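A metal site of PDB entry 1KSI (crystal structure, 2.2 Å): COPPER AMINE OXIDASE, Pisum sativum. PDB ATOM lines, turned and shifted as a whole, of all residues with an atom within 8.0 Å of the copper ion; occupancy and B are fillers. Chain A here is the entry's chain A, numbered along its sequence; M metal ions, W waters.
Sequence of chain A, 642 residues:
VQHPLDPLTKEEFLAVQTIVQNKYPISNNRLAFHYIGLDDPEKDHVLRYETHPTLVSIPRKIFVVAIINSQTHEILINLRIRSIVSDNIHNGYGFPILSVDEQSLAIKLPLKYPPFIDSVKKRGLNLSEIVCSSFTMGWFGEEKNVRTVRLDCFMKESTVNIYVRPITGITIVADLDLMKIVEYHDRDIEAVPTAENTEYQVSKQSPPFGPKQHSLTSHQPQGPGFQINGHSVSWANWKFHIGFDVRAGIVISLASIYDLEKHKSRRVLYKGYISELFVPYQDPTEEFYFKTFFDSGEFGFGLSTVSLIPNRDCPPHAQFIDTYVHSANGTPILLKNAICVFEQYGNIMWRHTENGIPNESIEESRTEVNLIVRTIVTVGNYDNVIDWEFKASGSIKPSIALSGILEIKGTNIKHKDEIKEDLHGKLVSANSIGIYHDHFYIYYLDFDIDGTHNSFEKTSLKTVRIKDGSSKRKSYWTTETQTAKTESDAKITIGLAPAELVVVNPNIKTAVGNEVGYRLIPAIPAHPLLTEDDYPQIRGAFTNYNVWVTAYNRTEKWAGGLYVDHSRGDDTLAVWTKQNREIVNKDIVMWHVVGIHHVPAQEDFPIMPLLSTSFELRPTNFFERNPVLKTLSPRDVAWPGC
The copper ion is bound by water W1, a ring nitrogen (NE2) of His 439, a ring nitrogen (NE2) of His 437, a ring nitrogen (ND1) of His 598 and water W2.
The backbone carbonyl oxygen (O) of His 439 sits at hydrogen-bond distance from the backbone NH (N) of Ile 596, 2.9 Å away. ND1 of His 437 lies within hydrogen-bond range of O of Ile 435. OD2 of Asp 604 sits at hydrogen-bond distance from NE2 of His 598, at 2.7 Å.
Of the 23 residues printed, 3 come within 4 Å of the copper ion.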
ATOM      1  N   VAL A 279      23.809 -20.607   0.041  1.00  0.00           N
ATOM      2  CA  VAL A 279      23.978 -21.731  -0.867  1.00  0.00           C
ATOM      3  C   VAL A 279      25.384 -22.307  -0.768  1.00  0.00           C
ATOM      4  O   VAL A 279      26.139 -22.087  -1.708  1.00  0.00           O
ATOM      5  CB  VAL A 279      23.718 -21.252  -2.304  1.00  0.00           C
ATOM      6  CG1 VAL A 279      23.575 -22.369  -3.338  1.00  0.00           C
ATOM      7  CG2 VAL A 279      22.479 -20.371  -2.314  1.00  0.00           C
ATOM      8  N   TYR A 281      28.487 -24.847  -0.967  1.00  0.00           N
ATOM      9  CA  TYR A 281      28.946 -26.007  -1.701  1.00  0.00           C
ATOM     10  C   TYR A 281      29.741 -26.877  -0.743  1.00  0.00           C
ATOM     11  O   TYR A 281      30.164 -26.504   0.355  1.00  0.00           O
ATOM     12  CB  TYR A 281      29.672 -25.577  -2.977  1.00  0.00           C
ATOM     13  CG  TYR A 281      28.684 -25.239  -4.071  1.00  0.00           C
ATOM     14  CD1 TYR A 281      27.868 -24.126  -3.963  1.00  0.00           C
ATOM     15  CD2 TYR A 281      28.558 -26.086  -5.145  1.00  0.00           C
ATOM     16  CE1 TYR A 281      26.927 -23.855  -4.916  1.00  0.00           C
ATOM     17  CE2 TYR A 281      27.590 -25.828  -6.120  1.00  0.00           C
ATOM     18  CZ  TYR A 281      26.786 -24.705  -5.965  1.00  0.00           C
ATOM     19  OH  TYR A 281      25.847 -24.461  -6.970  1.00  0.00           O
ATOM     20  N   ASN A 381      23.443 -18.860 -12.341  1.00  0.00           N
ATOM     21  CA  ASN A 381      22.950 -20.105 -12.914  1.00  0.00           C
ATOM     22  C   ASN A 381      21.670 -20.534 -12.187  1.00  0.00           C
ATOM     23  O   ASN A 381      21.050 -21.364 -12.816  1.00  0.00           O
ATOM     24  CB  ASN A 381      24.032 -21.170 -12.809  1.00  0.00           C
ATOM     25  CG  ASN A 381      24.446 -21.457 -11.395  1.00  0.00           C
ATOM     26  OD1 ASN A 381      24.830 -20.631 -10.564  1.00  0.00           O
ATOM     27  ND2 ASN A 381      24.318 -22.748 -11.054  1.00  0.00           N
ATOM     28  N   TPQ A 382      21.334 -20.023 -11.028  1.00  0.00           N
ATOM     29  CA  TPQ A 382      20.208 -20.254 -10.183  1.00  0.00           C
ATOM     30  CB  TPQ A 382      20.391 -19.988  -8.671  1.00  0.00           C
ATOM     31  C   TPQ A 382      18.938 -19.421 -10.457  1.00  0.00           C
ATOM     32  O   TPQ A 382      19.084 -18.222 -10.354  1.00  0.00           O
ATOM     33  C1  TPQ A 382      21.688 -20.401  -8.021  1.00  0.00           C
ATOM     34  C2  TPQ A 382      22.268 -19.541  -7.059  1.00  0.00           C
ATOM     35  O2  TPQ A 382      21.624 -18.421  -6.673  1.00  0.00           O
ATOM     36  C3  TPQ A 382      23.495 -19.811  -6.435  1.00  0.00           C
ATOM     37  C4  TPQ A 382      24.144 -20.996  -6.794  1.00  0.00           C
ATOM     38  O4  TPQ A 382      25.334 -21.343  -6.192  1.00  0.00           O
ATOM     39  C5  TPQ A 382      23.570 -21.887  -7.717  1.00  0.00           C
ATOM     40  O5  TPQ A 382      24.278 -22.994  -7.975  1.00  0.00           O
ATOM     41  C6  TPQ A 382      22.346 -21.603  -8.339  1.00  0.00           C
ATOM     42  N   LEU A 402      12.782 -24.033  -7.456  1.00  0.00           N
ATOM     43  CA  LEU A 402      14.119 -23.953  -8.004  1.00  0.00           C
ATOM     44  C   LEU A 402      14.204 -24.461  -9.424  1.00  0.00           C
ATOM     45  O   LEU A 402      13.662 -25.549  -9.694  1.00  0.00           O
ATOM     46  CB  LEU A 402      15.092 -24.823  -7.186  1.00  0.00           C
ATOM     47  CG  LEU A 402      15.134 -24.681  -5.666  1.00  0.00           C
ATOM     48  CD1 LEU A 402      16.404 -25.174  -4.995  1.00  0.00           C
ATOM     49  CD2 LEU A 402      14.949 -23.242  -5.218  1.00  0.00           C
ATOM     50  N   SER A 403      14.767 -23.719 -10.352  1.00  0.00           N
ATOM     51  CA  SER A 403      15.068 -24.159 -11.715  1.00  0.00           C
ATOM     52  C   SER A 403      16.479 -23.636 -12.125  1.00  0.00           C
ATOM     53  O   SER A 403      17.271 -23.322 -11.215  1.00  0.00           O
ATOM     54  CB  SER A 403      14.027 -23.787 -12.751  1.00  0.00           C
ATOM     55  OG  SER A 403      14.349 -24.464 -13.984  1.00  0.00           O
ATOM     56  N   ILE A 405      20.464 -23.994 -13.825  1.00  0.00           N
ATOM     57  CA  ILE A 405      21.535 -24.875 -14.328  1.00  0.00           C
ATOM     58  C   ILE A 405      22.481 -25.293 -13.241  1.00  0.00           C
ATOM     59  O   ILE A 405      22.846 -24.444 -12.399  1.00  0.00           O
ATOM     60  CB  ILE A 405      22.349 -24.165 -15.443  1.00  0.00           C
ATOM     61  CG1 ILE A 405      21.353 -23.887 -16.591  1.00  0.00           C
ATOM     62  CG2 ILE A 405      23.580 -24.930 -15.931  1.00  0.00           C
ATOM     63  CD1 ILE A 405      21.491 -22.396 -16.950  1.00  0.00           C
ATOM     64  N   LEU A 406      22.862 -26.553 -13.273  1.00  0.00           N
ATOM     65  CA  LEU A 406      23.853 -27.011 -12.308  1.00  0.00           C
ATOM     66  C   LEU A 406      25.225 -26.304 -12.521  1.00  0.00           C
ATOM     67  O   LEU A 406      25.687 -26.096 -13.652  1.00  0.00           O
ATOM     68  CB  LEU A 406      24.150 -28.510 -12.464  1.00  0.00           C
ATOM     69  CG  LEU A 406      23.079 -29.558 -12.058  1.00  0.00           C
ATOM     70  CD1 LEU A 406      23.542 -30.932 -12.517  1.00  0.00           C
ATOM     71  CD2 LEU A 406      22.803 -29.488 -10.563  1.00  0.00           C
ATOM     72  N   GLU A 407      25.804 -25.993 -11.361  1.00  0.00           N
ATOM     73  CA  GLU A 407      27.205 -25.565 -11.359  1.00  0.00           C
ATOM     74  C   GLU A 407      28.040 -26.824 -11.590  1.00  0.00           C
ATOM     75  O   GLU A 407      28.057 -27.675 -10.681  1.00  0.00           O
ATOM     76  CB  GLU A 407      27.493 -24.975  -9.970  1.00  0.00           C
ATOM     77  CG  GLU A 407      28.988 -24.843  -9.690  1.00  0.00           C
ATOM     78  CD  GLU A 407      29.450 -23.417  -9.900  1.00  0.00           C
ATOM     79  OE1 GLU A 407      28.831 -22.607 -10.620  1.00  0.00           O
ATOM     80  OE2 GLU A 407      30.506 -23.055  -9.323  1.00  0.00           O
ATOM     81  N   ILE A 435      28.281 -30.764  -8.230  1.00  0.00           N
ATOM     82  CA  ILE A 435      28.805 -30.710  -6.855  1.00  0.00           C
ATOM     83  C   ILE A 435      27.670 -30.663  -5.833  1.00  0.00           C
ATOM     84  O   ILE A 435      26.668 -29.986  -6.176  1.00  0.00           O
ATOM     85  CB  ILE A 435      29.697 -29.427  -6.707  1.00  0.00           C
ATOM     86  CG1 ILE A 435      30.837 -29.471  -7.746  1.00  0.00           C
ATOM     87  CG2 ILE A 435      30.227 -29.287  -5.292  1.00  0.00           C
ATOM     88  CD1 ILE A 435      31.760 -30.690  -7.449  1.00  0.00           C
ATOM     89  N   TYR A 436      27.827 -31.280  -4.659  1.00  0.00           N
ATOM     90  CA  TYR A 436      26.783 -31.229  -3.659  1.00  0.00           C
ATOM     91  C   TYR A 436      26.706 -29.826  -3.030  1.00  0.00           C
ATOM     92  O   TYR A 436      27.767 -29.282  -2.652  1.00  0.00           O
ATOM     93  CB  TYR A 436      26.990 -32.135  -2.442  1.00  0.00           C
ATOM     94  CG  TYR A 436      27.292 -33.570  -2.797  1.00  0.00           C
ATOM     95  CD1 TYR A 436      26.413 -34.308  -3.608  1.00  0.00           C
ATOM     96  CD2 TYR A 436      28.419 -34.202  -2.286  1.00  0.00           C
ATOM     97  CE1 TYR A 436      26.699 -35.629  -3.936  1.00  0.00           C
ATOM     98  CE2 TYR A 436      28.716 -35.522  -2.623  1.00  0.00           C
ATOM     99  CZ  TYR A 436      27.831 -36.224  -3.429  1.00  0.00           C
ATOM    100  OH  TYR A 436      28.123 -37.547  -3.750  1.00  0.00           O
ATOM    101  N   HIS A 437      25.505 -29.364  -2.827  1.00  0.00           N
ATOM    102  CA  HIS A 437      25.307 -28.137  -2.103  1.00  0.00           C
ATOM    103  C   HIS A 437      23.905 -28.072  -1.501  1.00  0.00           C
ATOM    104  O   HIS A 437      23.060 -28.899  -1.826  1.00  0.00           O
ATOM    105  CB  HIS A 437      25.409 -26.963  -3.107  1.00  0.00           C
ATOM    106  CG  HIS A 437      24.454 -27.180  -4.237  1.00  0.00           C
ATOM    107  ND1 HIS A 437      24.687 -28.161  -5.177  1.00  0.00           N
ATOM    108  CD2 HIS A 437      23.284 -26.625  -4.562  1.00  0.00           C
ATOM    109  CE1 HIS A 437      23.751 -28.141  -6.129  1.00  0.00           C
ATOM    110  NE2 HIS A 437      22.860 -27.241  -5.720  1.00  0.00           N
ATOM    111  N   ASP A 438      23.669 -27.047  -0.694  1.00  0.00           N
ATOM    112  CA  ASP A 438      22.436 -26.752  -0.031  1.00  0.00           C
ATOM    113  C   ASP A 438      21.892 -25.411  -0.514  1.00  0.00           C
ATOM    114  O   ASP A 438      22.645 -24.587  -1.056  1.00  0.00           O
ATOM    115  CB  ASP A 438      22.572 -26.655   1.488  1.00  0.00           C
ATOM    116  CG  ASP A 438      23.274 -27.898   2.006  1.00  0.00           C
ATOM    117  OD1 ASP A 438      22.985 -29.030   1.531  1.00  0.00           O
ATOM    118  OD2 ASP A 438      24.137 -27.775   2.896  1.00  0.00           O
ATOM    119  N   HIS A 439      20.598 -25.265  -0.305  1.00  0.00           N
ATOM    120  CA  HIS A 439      19.910 -24.010  -0.544  1.00  0.00           C
ATOM    121  C   HIS A 439      19.112 -23.683   0.714  1.00  0.00           C
ATOM    122  O   HIS A 439      18.233 -24.460   1.066  1.00  0.00           O
ATOM    123  CB  HIS A 439      19.026 -23.932  -1.739  1.00  0.00           C
ATOM    124  CG  HIS A 439      19.582 -24.379  -3.065  1.00  0.00           C
ATOM    125  ND1 HIS A 439      19.729 -23.542  -4.174  1.00  0.00           N
ATOM    126  CD2 HIS A 439      19.983 -25.633  -3.453  1.00  0.00           C
ATOM    127  CE1 HIS A 439      20.193 -24.254  -5.187  1.00  0.00           C
ATOM    128  NE2 HIS A 439      20.340 -25.517  -4.786  1.00  0.00           N
ATOM    129  N   TYR A 441      16.846 -20.553   2.717  1.00  0.00           N
ATOM    130  CA  TYR A 441      16.174 -19.289   2.659  1.00  0.00           C
ATOM    131  C   TYR A 441      15.714 -18.926   4.063  1.00  0.00           C
ATOM    132  O   TYR A 441      15.335 -19.876   4.757  1.00  0.00           O
ATOM    133  CB  TYR A 441      14.965 -19.248   1.759  1.00  0.00           C
ATOM    134  CG  TYR A 441      15.285 -19.809   0.363  1.00  0.00           C
ATOM    135  CD1 TYR A 441      15.581 -21.166   0.164  1.00  0.00           C
ATOM    136  CD2 TYR A 441      15.206 -18.957  -0.738  1.00  0.00           C
ATOM    137  CE1 TYR A 441      15.809 -21.685  -1.111  1.00  0.00           C
ATOM    138  CE2 TYR A 441      15.435 -19.467  -2.023  1.00  0.00           C
ATOM    139  CZ  TYR A 441      15.743 -20.795  -2.196  1.00  0.00           C
ATOM    140  OH  TYR A 441      16.005 -21.246  -3.474  1.00  0.00           O
ATOM    141  N   ILE A 596      16.959 -27.092   1.428  1.00  0.00           N
ATOM    142  CA  ILE A 596      17.060 -28.278   0.624  1.00  0.00           C
ATOM    143  C   ILE A 596      18.478 -28.794   0.434  1.00  0.00           C
ATOM    144  O   ILE A 596      19.338 -27.966   0.061  1.00  0.00           O
ATOM    145  CB  ILE A 596      16.646 -27.879  -0.832  1.00  0.00           C
ATOM    146  CG1 ILE A 596      15.420 -27.004  -0.759  1.00  0.00           C
ATOM    147  CG2 ILE A 596      16.487 -29.143  -1.646  1.00  0.00           C
ATOM    148  CD1 ILE A 596      14.562 -26.796  -1.998  1.00  0.00           C
ATOM    149  N   HIS A 597      18.750 -30.074   0.612  1.00  0.00           N
ATOM    150  CA  HIS A 597      20.058 -30.666   0.379  1.00  0.00           C
ATOM    151  C   HIS A 597      19.996 -31.169  -1.049  1.00  0.00           C
ATOM    152  O   HIS A 597      19.007 -31.826  -1.367  1.00  0.00           O
ATOM    153  CB  HIS A 597      20.407 -31.807   1.280  1.00  0.00           C
ATOM    154  CG  HIS A 597      20.461 -31.407   2.720  1.00  0.00           C
ATOM    155  ND1 HIS A 597      21.363 -30.506   3.200  1.00  0.00           N
ATOM    156  CD2 HIS A 597      19.774 -31.831   3.801  1.00  0.00           C
ATOM    157  CE1 HIS A 597      21.228 -30.377   4.513  1.00  0.00           C
ATOM    158  NE2 HIS A 597      20.265 -31.190   4.897  1.00  0.00           N
ATOM    159  N   HIS A 598      20.941 -30.776  -1.885  1.00  0.00           N
ATOM    160  CA  HIS A 598      20.829 -31.077  -3.294  1.00  0.00           C
ATOM    161  C   HIS A 598      21.926 -32.027  -3.734  1.00  0.00           C
ATOM    162  O   HIS A 598      23.101 -31.648  -3.802  1.00  0.00           O
ATOM    163  CB  HIS A 598      20.828 -29.843  -4.187  1.00  0.00           C
ATOM    164  CG  HIS A 598      20.554 -30.045  -5.653  1.00  0.00           C
ATOM    165  ND1 HIS A 598      20.440 -29.006  -6.574  1.00  0.00           N
ATOM    166  CD2 HIS A 598      20.322 -31.155  -6.376  1.00  0.00           C
ATOM    167  CE1 HIS A 598      20.164 -29.512  -7.752  1.00  0.00           C
ATOM    168  NE2 HIS A 598      20.083 -30.830  -7.694  1.00  0.00           N
ATOM    169  N   VAL A 599      21.495 -33.271  -4.019  1.00  0.00           N
ATOM    170  CA  VAL A 599      22.308 -34.305  -4.629  1.00  0.00           C
ATOM    171  C   VAL A 599      21.890 -34.284  -6.095  1.00  0.00           C
ATOM    172  O   VAL A 599      20.728 -34.609  -6.458  1.00  0.00           O
ATOM    173  CB  VAL A 599      22.079 -35.686  -4.028  1.00  0.00           C
ATOM    174  CG1 VAL A 599      22.976 -36.708  -4.692  1.00  0.00           C
ATOM    175  CG2 VAL A 599      22.287 -35.698  -2.502  1.00  0.00           C
ATOM    176  N   PRO A 600      22.797 -33.787  -6.942  1.00  0.00           N
ATOM    177  CA  PRO A 600      22.450 -33.670  -8.367  1.00  0.00           C
ATOM    178  C   PRO A 600      22.190 -35.055  -8.987  1.00  0.00           C
ATOM    179  O   PRO A 600      22.763 -36.072  -8.562  1.00  0.00           O
ATOM    180  CB  PRO A 600      23.655 -32.934  -8.960  1.00  0.00           C
ATOM    181  CG  PRO A 600      24.141 -32.159  -7.770  1.00  0.00           C
ATOM    182  CD  PRO A 600      24.101 -33.149  -6.616  1.00  0.00           C
ATOM    183  N   ASP A 604      18.511 -33.274 -13.864  1.00  0.00           N
ATOM    184  CA  ASP A 604      18.889 -31.914 -13.532  1.00  0.00           C
ATOM    185  C   ASP A 604      19.776 -31.279 -14.627  1.00  0.00           C
ATOM    186  O   ASP A 604      19.970 -30.086 -14.567  1.00  0.00           O
ATOM    187  CB  ASP A 604      19.760 -31.932 -12.264  1.00  0.00           C
ATOM    188  CG  ASP A 604      19.008 -32.190 -10.983  1.00  0.00           C
ATOM    189  OD1 ASP A 604      17.777 -32.156 -11.116  1.00  0.00           O
ATOM    190  OD2 ASP A 604      19.563 -32.360  -9.881  1.00  0.00           O
ATOM    191  N   MET A 608      17.332 -27.716 -15.173  1.00  0.00           N
ATOM    192  CA  MET A 608      16.622 -28.531 -14.200  1.00  0.00           C
ATOM    193  C   MET A 608      15.129 -28.372 -14.060  1.00  0.00           C
ATOM    194  O   MET A 608      14.551 -27.293 -13.979  1.00  0.00           O
ATOM    195  CB  MET A 608      17.438 -28.359 -12.951  1.00  0.00           C
ATOM    196  CG  MET A 608      16.653 -27.859 -11.793  1.00  0.00           C
ATOM    197  SD  MET A 608      17.677 -28.009 -10.307  1.00  0.00           S
ATOM    198  CE  MET A 608      16.349 -27.989  -9.074  1.00  0.00           C
ATOM    199  N   LEU A 611      11.748 -27.955  -8.890  1.00  0.00           N
ATOM    200  CA  LEU A 611      11.756 -28.570  -7.641  1.00  0.00           C
ATOM    201  C   LEU A 611      11.198 -27.492  -6.688  1.00  0.00           C
ATOM    202  O   LEU A 611      11.688 -26.388  -6.587  1.00  0.00           O
ATOM    203  CB  LEU A 611      13.079 -29.009  -7.093  1.00  0.00           C
ATOM    204  CG  LEU A 611      12.855 -29.777  -5.768  1.00  0.00           C
ATOM    205  CD1 LEU A 611      12.625 -31.250  -6.104  1.00  0.00           C
ATOM    206  CD2 LEU A 611      14.082 -29.675  -4.899  1.00  0.00           C
HETATM  207 CU    CU M   1      20.838 -26.890  -6.260  1.00  0.00          CU
HETATM  208  O   HOH W   1      19.298 -26.416  -7.376  1.00  0.00           O
HETATM  209  O   HOH W   2      21.481 -26.102  -8.485  1.00  0.00           O
